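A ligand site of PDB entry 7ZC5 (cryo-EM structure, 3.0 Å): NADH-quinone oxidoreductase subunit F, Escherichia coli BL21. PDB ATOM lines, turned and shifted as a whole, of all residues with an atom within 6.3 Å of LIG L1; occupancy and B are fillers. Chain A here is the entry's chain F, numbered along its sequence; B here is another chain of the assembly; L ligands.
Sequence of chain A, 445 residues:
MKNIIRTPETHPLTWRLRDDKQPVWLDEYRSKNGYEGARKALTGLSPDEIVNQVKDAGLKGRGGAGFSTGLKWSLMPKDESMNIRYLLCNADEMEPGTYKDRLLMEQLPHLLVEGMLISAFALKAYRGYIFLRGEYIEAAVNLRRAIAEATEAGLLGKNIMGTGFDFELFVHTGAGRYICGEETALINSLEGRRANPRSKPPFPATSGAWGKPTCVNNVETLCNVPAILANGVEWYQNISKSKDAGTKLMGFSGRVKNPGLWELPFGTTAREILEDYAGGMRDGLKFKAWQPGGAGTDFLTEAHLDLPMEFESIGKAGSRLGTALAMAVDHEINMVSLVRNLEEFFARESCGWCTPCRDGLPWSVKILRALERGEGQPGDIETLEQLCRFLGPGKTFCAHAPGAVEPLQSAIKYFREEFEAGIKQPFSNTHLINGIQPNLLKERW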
ATOM      1  N   ILE A 179      31.744 -19.804  14.997  1.00  0.00           N
ATOM      2  CA  ILE A 179      31.165 -20.952  14.316  1.00  0.00           C
ATOM      3  C   ILE A 179      32.214 -22.016  13.993  1.00  0.00           C
ATOM      4  O   ILE A 179      31.859 -23.170  13.750  1.00  0.00           O
ATOM      5  CB  ILE A 179      30.404 -20.479  13.060  1.00  0.00           C
ATOM      6  CG1 ILE A 179      29.404 -21.530  12.578  1.00  0.00           C
ATOM      7  CG2 ILE A 179      31.371 -20.107  11.963  1.00  0.00           C
ATOM      8  CD1 ILE A 179      28.591 -22.146  13.666  1.00  0.00           C
ATOM      9  N   ASN A 196      31.368 -22.848   7.120  1.00  0.00           N
ATOM     10  CA  ASN A 196      29.963 -23.220   7.176  1.00  0.00           C
ATOM     11  C   ASN A 196      29.848 -24.667   7.624  1.00  0.00           C
ATOM     12  O   ASN A 196      30.629 -25.519   7.184  1.00  0.00           O
ATOM     13  CB  ASN A 196      29.314 -23.054   5.805  1.00  0.00           C
ATOM     14  CG  ASN A 196      29.371 -21.637   5.302  1.00  0.00           C
ATOM     15  OD1 ASN A 196      30.049 -21.359   4.319  1.00  0.00           O
ATOM     16  ND2 ASN A 196      28.659 -20.739   5.958  1.00  0.00           N
ATOM     17  N   PRO A 197      28.892 -24.987   8.496  1.00  0.00           N
ATOM     18  CA  PRO A 197      28.718 -26.363   8.935  1.00  0.00           C
ATOM     19  C   PRO A 197      28.205 -27.268   7.826  1.00  0.00           C
ATOM     20  O   PRO A 197      27.883 -26.848   6.713  1.00  0.00           O
ATOM     21  CB  PRO A 197      27.703 -26.247  10.070  1.00  0.00           C
ATOM     22  CG  PRO A 197      27.114 -24.919   9.941  1.00  0.00           C
ATOM     23  CD  PRO A 197      28.126 -24.050   9.322  1.00  0.00           C
ATOM     24  N   GLU A 349      28.071 -13.469  14.956  1.00  0.00           N
ATOM     25  CA  GLU A 349      28.863 -14.674  14.810  1.00  0.00           C
ATOM     26  C   GLU A 349      28.150 -15.716  13.957  1.00  0.00           C
ATOM     27  O   GLU A 349      28.598 -16.864  13.906  1.00  0.00           O
ATOM     28  CB  GLU A 349      29.207 -15.261  16.178  1.00  0.00           C
ATOM     29  CG  GLU A 349      30.221 -14.433  16.936  1.00  0.00           C
ATOM     30  CD  GLU A 349      31.485 -14.152  16.149  1.00  0.00           C
ATOM     31  OE1 GLU A 349      32.018 -15.077  15.514  1.00  0.00           O
ATOM     32  OE2 GLU A 349      31.947 -12.993  16.173  1.00  0.00           O
ATOM     33  N   SER A 350      27.064 -15.338  13.308  1.00  0.00           N
ATOM     34  CA  SER A 350      26.408 -16.204  12.337  1.00  0.00           C
ATOM     35  C   SER A 350      27.314 -16.436  11.137  1.00  0.00           C
ATOM     36  O   SER A 350      28.141 -15.583  10.776  1.00  0.00           O
ATOM     37  CB  SER A 350      25.097 -15.577  11.887  1.00  0.00           C
ATOM     38  OG  SER A 350      24.579 -16.229  10.744  1.00  0.00           O
ATOM     39  N   CYS A 351      27.191 -17.601  10.528  1.00  0.00           N
ATOM     40  CA  CYS A 351      27.997 -17.894   9.358  1.00  0.00           C
ATOM     41  C   CYS A 351      27.332 -17.465   8.058  1.00  0.00           C
ATOM     42  O   CYS A 351      28.003 -17.432   7.027  1.00  0.00           O
ATOM     43  CB  CYS A 351      28.337 -19.380   9.324  1.00  0.00           C
ATOM     44  SG  CYS A 351      27.107 -20.457   8.635  1.00  0.00           S
ATOM     45  N   GLY A 352      26.053 -17.111   8.092  1.00  0.00           N
ATOM     46  CA  GLY A 352      25.331 -16.637   6.942  1.00  0.00           C
ATOM     47  C   GLY A 352      24.742 -17.706   6.056  1.00  0.00           C
ATOM     48  O   GLY A 352      24.178 -17.364   5.014  1.00  0.00           O
ATOM     49  N   TRP A 353      24.868 -18.972   6.428  1.00  0.00           N
ATOM     50  CA  TRP A 353      24.424 -20.054   5.555  1.00  0.00           C
ATOM     51  C   TRP A 353      22.904 -20.118   5.480  1.00  0.00           C
ATOM     52  O   TRP A 353      22.333 -20.165   4.389  1.00  0.00           O
ATOM     53  CB  TRP A 353      24.998 -21.367   6.046  1.00  0.00           C
ATOM     54  CG  TRP A 353      24.527 -22.571   5.339  1.00  0.00           C
ATOM     55  CD1 TRP A 353      23.704 -23.524   5.837  1.00  0.00           C
ATOM     56  CD2 TRP A 353      24.850 -22.959   4.016  1.00  0.00           C
ATOM     57  NE1 TRP A 353      23.499 -24.495   4.898  1.00  0.00           N
ATOM     58  CE2 TRP A 353      24.190 -24.174   3.762  1.00  0.00           C
ATOM     59  CE3 TRP A 353      25.632 -22.406   3.004  1.00  0.00           C
ATOM     60  CZ2 TRP A 353      24.289 -24.843   2.554  1.00  0.00           C
ATOM     61  CZ3 TRP A 353      25.735 -23.064   1.804  1.00  0.00           C
ATOM     62  CH2 TRP A 353      25.063 -24.261   1.582  1.00  0.00           C
ATOM     63  N   CYS A 354      22.239 -20.114   6.618  1.00  0.00           N
ATOM     64  CA  CYS A 354      20.822 -20.434   6.659  1.00  0.00           C
ATOM     65  C   CYS A 354      19.986 -19.244   7.095  1.00  0.00           C
ATOM     66  O   CYS A 354      20.415 -18.437   7.916  1.00  0.00           O
ATOM     67  CB  CYS A 354      20.581 -21.662   7.536  1.00  0.00           C
ATOM     68  SG  CYS A 354      20.446 -21.431   9.274  1.00  0.00           S
ATOM     69  N   THR A 355      18.810 -19.131   6.491  1.00  0.00           N
ATOM     70  CA  THR A 355      17.972 -17.932   6.617  1.00  0.00           C
ATOM     71  C   THR A 355      17.520 -17.598   8.036  1.00  0.00           C
ATOM     72  O   THR A 355      17.603 -16.407   8.393  1.00  0.00           O
ATOM     73  CB  THR A 355      16.777 -18.053   5.656  1.00  0.00           C
ATOM     74  OG1 THR A 355      17.243 -18.190   4.320  1.00  0.00           O
ATOM     75  CG2 THR A 355      15.873 -16.839   5.742  1.00  0.00           C
ATOM     76  N   PRO A 356      17.042 -18.533   8.871  1.00  0.00           N
ATOM     77  CA  PRO A 356      16.530 -18.102  10.188  1.00  0.00           C
ATOM     78  C   PRO A 356      17.564 -17.432  11.066  1.00  0.00           C
ATOM     79  O   PRO A 356      17.310 -16.343  11.569  1.00  0.00           O
ATOM     80  CB  PRO A 356      16.018 -19.410  10.802  1.00  0.00           C
ATOM     81  CG  PRO A 356      15.727 -20.241   9.688  1.00  0.00           C
ATOM     82  CD  PRO A 356      16.799 -19.970   8.715  1.00  0.00           C
ATOM     83  N   CYS A 357      18.757 -18.000  11.202  1.00  0.00           N
ATOM     84  CA  CYS A 357      19.783 -17.352  12.003  1.00  0.00           C
ATOM     85  C   CYS A 357      20.264 -16.065  11.356  1.00  0.00           C
ATOM     86  O   CYS A 357      20.170 -14.996  11.962  1.00  0.00           O
ATOM     87  CB  CYS A 357      20.919 -18.343  12.250  1.00  0.00           C
ATOM     88  SG  CYS A 357      22.516 -17.811  12.843  1.00  0.00           S
ATOM     89  N   ARG A 358      20.627 -16.136  10.063  1.00  0.00           N
ATOM     90  CA  ARG A 358      21.240 -15.007   9.349  1.00  0.00           C
ATOM     91  C   ARG A 358      20.320 -13.794   9.294  1.00  0.00           C
ATOM     92  O   ARG A 358      20.775 -12.658   9.478  1.00  0.00           O
ATOM     93  CB  ARG A 358      21.620 -15.433   7.926  1.00  0.00           C
ATOM     94  CG  ARG A 358      21.726 -14.296   6.924  1.00  0.00           C
ATOM     95  CD  ARG A 358      21.954 -14.774   5.520  1.00  0.00           C
ATOM     96  NE  ARG A 358      20.703 -15.063   4.841  1.00  0.00           N
ATOM     97  CZ  ARG A 358      20.346 -16.259   4.409  1.00  0.00           C
ATOM     98  NH1 ARG A 358      21.123 -17.305   4.573  1.00  0.00           N
ATOM     99  NH2 ARG A 358      19.187 -16.400   3.784  1.00  0.00           N
ATOM    100  N   LEU A 361      18.223 -13.319  13.554  1.00  0.00           N
ATOM    101  CA  LEU A 361      18.896 -12.792  14.722  1.00  0.00           C
ATOM    102  C   LEU A 361      19.125 -11.279  14.654  1.00  0.00           C
ATOM    103  O   LEU A 361      19.014 -10.625  15.702  1.00  0.00           O
ATOM    104  CB  LEU A 361      20.212 -13.542  14.941  1.00  0.00           C
ATOM    105  CG  LEU A 361      20.051 -14.978  15.407  1.00  0.00           C
ATOM    106  CD1 LEU A 361      21.379 -15.634  15.589  1.00  0.00           C
ATOM    107  CD2 LEU A 361      19.276 -14.999  16.705  1.00  0.00           C
ATOM    108  N   THR A 396      16.879 -24.462  11.947  1.00  0.00           N
ATOM    109  CA  THR A 396      18.087 -23.922  11.353  1.00  0.00           C
ATOM    110  C   THR A 396      19.024 -25.053  10.950  1.00  0.00           C
ATOM    111  O   THR A 396      18.856 -26.202  11.337  1.00  0.00           O
ATOM    112  CB  THR A 396      18.791 -22.964  12.313  1.00  0.00           C
ATOM    113  OG1 THR A 396      19.195 -23.688  13.481  1.00  0.00           O
ATOM    114  CG2 THR A 396      17.854 -21.875  12.711  1.00  0.00           C
ATOM    115  N   PHE A 397      20.038 -24.685  10.173  1.00  0.00           N
ATOM    116  CA  PHE A 397      20.959 -25.672   9.630  1.00  0.00           C
ATOM    117  C   PHE A 397      21.843 -26.267  10.721  1.00  0.00           C
ATOM    118  O   PHE A 397      22.119 -27.473  10.704  1.00  0.00           O
ATOM    119  CB  PHE A 397      21.794 -25.040   8.534  1.00  0.00           C
ATOM    120  CG  PHE A 397      22.590 -26.008   7.737  1.00  0.00           C
ATOM    121  CD1 PHE A 397      21.995 -26.764   6.748  1.00  0.00           C
ATOM    122  CD2 PHE A 397      23.938 -26.163   7.971  1.00  0.00           C
ATOM    123  CE1 PHE A 397      22.727 -27.647   6.014  1.00  0.00           C
ATOM    124  CE2 PHE A 397      24.680 -27.049   7.235  1.00  0.00           C
ATOM    125  CZ  PHE A 397      24.069 -27.790   6.257  1.00  0.00           C
ATOM    126  N   CYS A 398      22.297 -25.452  11.670  1.00  0.00           N
ATOM    127  CA  CYS A 398      23.089 -25.956  12.779  1.00  0.00           C
ATOM    128  C   CYS A 398      22.519 -25.462  14.109  1.00  0.00           C
ATOM    129  O   CYS A 398      21.443 -24.867  14.129  1.00  0.00           O
ATOM    130  CB  CYS A 398      24.555 -25.551  12.623  1.00  0.00           C
ATOM    131  SG  CYS A 398      25.037 -24.007  13.405  1.00  0.00           S
ATOM    132  N   ALA A 399      23.217 -25.713  15.213  1.00  0.00           N
ATOM    133  CA  ALA A 399      22.687 -25.413  16.530  1.00  0.00           C
ATOM    134  C   ALA A 399      23.196 -24.090  17.079  1.00  0.00           C
ATOM    135  O   ALA A 399      23.218 -23.894  18.295  1.00  0.00           O
ATOM    136  CB  ALA A 399      23.010 -26.550  17.493  1.00  0.00           C
ATOM    137  N   HIS A 400      23.612 -23.170  16.207  1.00  0.00           N
ATOM    138  CA  HIS A 400      24.000 -21.851  16.668  1.00  0.00           C
ATOM    139  C   HIS A 400      22.796 -21.029  17.097  1.00  0.00           C
ATOM    140  O   HIS A 400      22.830 -20.381  18.146  1.00  0.00           O
ATOM    141  CB  HIS A 400      24.760 -21.124  15.565  1.00  0.00           C
ATOM    142  CG  HIS A 400      25.058 -19.685  15.854  1.00  0.00           C
ATOM    143  ND1 HIS A 400      26.195 -19.277  16.509  1.00  0.00           N
ATOM    144  CD2 HIS A 400      24.375 -18.557  15.545  1.00  0.00           C
ATOM    145  CE1 HIS A 400      26.193 -17.964  16.599  1.00  0.00           C
ATOM    146  NE2 HIS A 400      25.105 -17.502  16.021  1.00  0.00           N
ATOM    147  N   ALA A 401      21.725 -21.058  16.315  1.00  0.00           N
ATOM    148  CA  ALA A 401      20.536 -20.260  16.569  1.00  0.00           C
ATOM    149  C   ALA A 401      19.607 -20.802  17.671  1.00  0.00           C
ATOM    150  O   ALA A 401      19.013 -19.987  18.386  1.00  0.00           O
ATOM    151  CB  ALA A 401      19.760 -20.069  15.272  1.00  0.00           C
ATOM    152  N   PRO A 402      19.417 -22.128  17.850  1.00  0.00           N
ATOM    153  CA  PRO A 402      18.703 -22.576  19.060  1.00  0.00           C
ATOM    154  C   PRO A 402      19.378 -22.144  20.344  1.00  0.00           C
ATOM    155  O   PRO A 402      18.706 -21.631  21.260  1.00  0.00           O
ATOM    156  CB  PRO A 402      18.693 -24.094  18.908  1.00  0.00           C
ATOM    157  CG  PRO A 402      18.713 -24.312  17.490  1.00  0.00           C
ATOM    158  CD  PRO A 402      19.573 -23.255  16.909  1.00  0.00           C
ATOM    159  N   HIS B 176      27.919 -13.081   8.576  1.00  0.00           N
ATOM    160  CA  HIS B 176      26.611 -13.297   9.158  1.00  0.00           C
ATOM    161  C   HIS B 176      25.394 -12.870   8.365  1.00  0.00           C
ATOM    162  O   HIS B 176      24.565 -13.711   8.014  1.00  0.00           O
ATOM    163  CB  HIS B 176      26.616 -12.506  10.461  1.00  0.00           C
ATOM    164  CG  HIS B 176      27.478 -11.281  10.382  1.00  0.00           C
ATOM    165  ND1 HIS B 176      27.029 -10.087   9.861  1.00  0.00           N
ATOM    166  CD2 HIS B 176      28.772 -11.081  10.713  1.00  0.00           C
ATOM    167  CE1 HIS B 176      28.005  -9.204   9.887  1.00  0.00           C
ATOM    168  NE2 HIS B 176      29.079  -9.778  10.400  1.00  0.00           N
HETATM  169 FE1  LIG L   1      22.556 -21.296  10.237  1.00  0.00          FE
HETATM  170 FE2  LIG L   1      23.599 -19.643  11.928  1.00  0.00          FE
HETATM  171 FE3  LIG L   1      24.419 -22.240  12.037  1.00  0.00          FE
HETATM  172 FE4  LIG L   1      25.267 -20.748  10.028  1.00  0.00          FE
HETATM  173  S1  LIG L   1      25.755 -20.379  12.247  1.00  0.00           S
HETATM  174  S2  LIG L   1      24.252 -22.801   9.808  1.00  0.00           S
HETATM  175  S3  LIG L   1      23.527 -19.311   9.661  1.00  0.00           S
HETATM  176  S4  LIG L   1      22.311 -21.467  12.517  1.00  0.00           S
HETATM  177  N1  LG2 L   2      32.741 -27.510  21.009  1.00  0.00           N
HETATM  178  C1  LG2 L   2      33.993 -27.168  21.463  1.00  0.00           C
HETATM  179  O1  LG2 L   2      34.642 -28.013  22.061  1.00  0.00           O
HETATM  180  N2  LG2 L   2      34.487 -25.909  21.261  1.00  0.00           N
HETATM  181  C2  LG2 L   2      33.726 -24.986  20.584  1.00  0.00           C
HETATM  182  O2  LG2 L   2      34.165 -23.859  20.401  1.00  0.00           O
HETATM  183  C3  LG2 L   2      32.475 -25.319  20.128  1.00  0.00           C
HETATM  184  N3  LG2 L   2      31.726 -24.396  19.459  1.00  0.00           N
HETATM  185  C4  LG2 L   2      30.492 -24.734  18.990  1.00  0.00           C
HETATM  186  C5  LG2 L   2      29.748 -23.782  18.315  1.00  0.00           C
HETATM  187  C6  LG2 L   2      28.489 -24.095  17.848  1.00  0.00           C
HETATM  188  C7  LG2 L   2      27.700 -23.062  17.120  1.00  0.00           C
HETATM  189  C8  LG2 L   2      27.984 -25.361  18.053  1.00  0.00           C
HETATM  190  C9  LG2 L   2      26.617 -25.712  17.552  1.00  0.00           C
HETATM  191  C10 LG2 L   2      28.724 -26.323  18.720  1.00  0.00           C
HETATM  192  C11 LG2 L   2      29.985 -26.010  19.197  1.00  0.00           C
HETATM  193  N4  LG2 L   2      30.745 -26.943  19.876  1.00  0.00           N
HETATM  194  C12 LG2 L   2      31.980 -26.587  20.332  1.00  0.00           C
HETATM  195  C13 LG2 L   2      30.270 -28.351  20.125  1.00  0.00           C
HETATM  196  C14 LG2 L   2      30.803 -29.264  19.014  1.00  0.00           C
HETATM  197  O3  LG2 L   2      29.856 -29.327  17.984  1.00  0.00           O
HETATM  198  C15 LG2 L   2      31.082 -30.684  19.489  1.00  0.00           C
HETATM  199  O4  LG2 L   2      29.981 -31.110  20.251  1.00  0.00           O
HETATM  200  C16 LG2 L   2      32.344 -30.739  20.335  1.00  0.00           C
HETATM  201  O5  LG2 L   2      33.284 -29.826  19.839  1.00  0.00           O
HETATM  202  C17 LG2 L   2      32.994 -32.110  20.396  1.00  0.00           C
HETATM  203  O6  LG2 L   2      32.165 -33.034  21.055  1.00  0.00           O
HETATM  204  P1  LG2 L   2      32.579 -33.600  22.499  1.00  0.00           P
HETATM  205  O7  LG2 L   2      31.765 -32.850  23.505  1.00  0.00           O
HETATM  206  O8  LG2 L   2      32.302 -35.069  22.591  1.00  0.00           O
HETATM  207  O9  LG2 L   2      34.033 -33.359  22.749  1.00  0.00           O
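The side-chain sulfur of Cys 357 binds an iron atom (FE2) of LIG L1 (2.3 Å). S2 of LIG L1 lies close to N of Cys 398, 3.8 Å away. FE3 of LIG L1 is bound by SG of Cys 398 (2.3 Å). A sulfur (S3) of LIG L1 lies close to the backbone NH of Cys 354. SG of Cys 354 binds FE1 of LIG L1. The backbone NH (N) of Cys 351 sits close to a sulfur (S1) of LIG L1 (3.6 Å). The side-chain sulfur (SG) of Cys 351 binds an iron atom (FE4) of LIG L1 (2.3 Å). The side-chain hydroxyl of Ser 350 lies close to a sulfur (S3) of LIG L1 (3.4 Å). S3 of LIG L1 lies close to N of Trp 353 (3.5 Å). The backbone NH (N) of Gly 352 lies close to a sulfur (S3) of LIG L1.
Ile 179 touches LIG L1. Pro 197 touches LIG L1. Thr 396 touches LIG L1. Phe 397 touches LIG L1. His 400 touches LIG L1 (CB to S1, 3.5 Å). Ala 401 touches LIG L1. 13 residues have an atom within 4 Å of LIG L1: Ile 179, Pro 197, Ser 350, Cys 351, Gly 352, Trp 353, Cys 354, Cys 357, Thr 396, Phe 397, Cys 398, His 400 and Ala 401.
O of Cys 398 sits at hydrogen-bond distance from OG1 of Thr 396 (2.6 Å). The side-chain sulfur (SG) of Cys 354 lies close to the backbone NH (N) of Phe 397. SG of Cys 351 lies close to N of Trp 353, at 3.5 Å. The side-chain sulfur of Cys 351 sits close to the side-chain amide nitrogen of Asn 196. The side-chain hydroxyl (OG) of Ser 350 is in hydrogen-bond range of the backbone NH (N) of Gly 352, at 3.2 Å. O of Ser 350 sits close to N of His 176 of chain B. O of Trp 353 sits at hydrogen-bond distance from NH1 of Arg 358 (3.1 Å). O of Gly 352 lies within hydrogen-bond range of NH1 of Arg 358 (3.1 Å).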
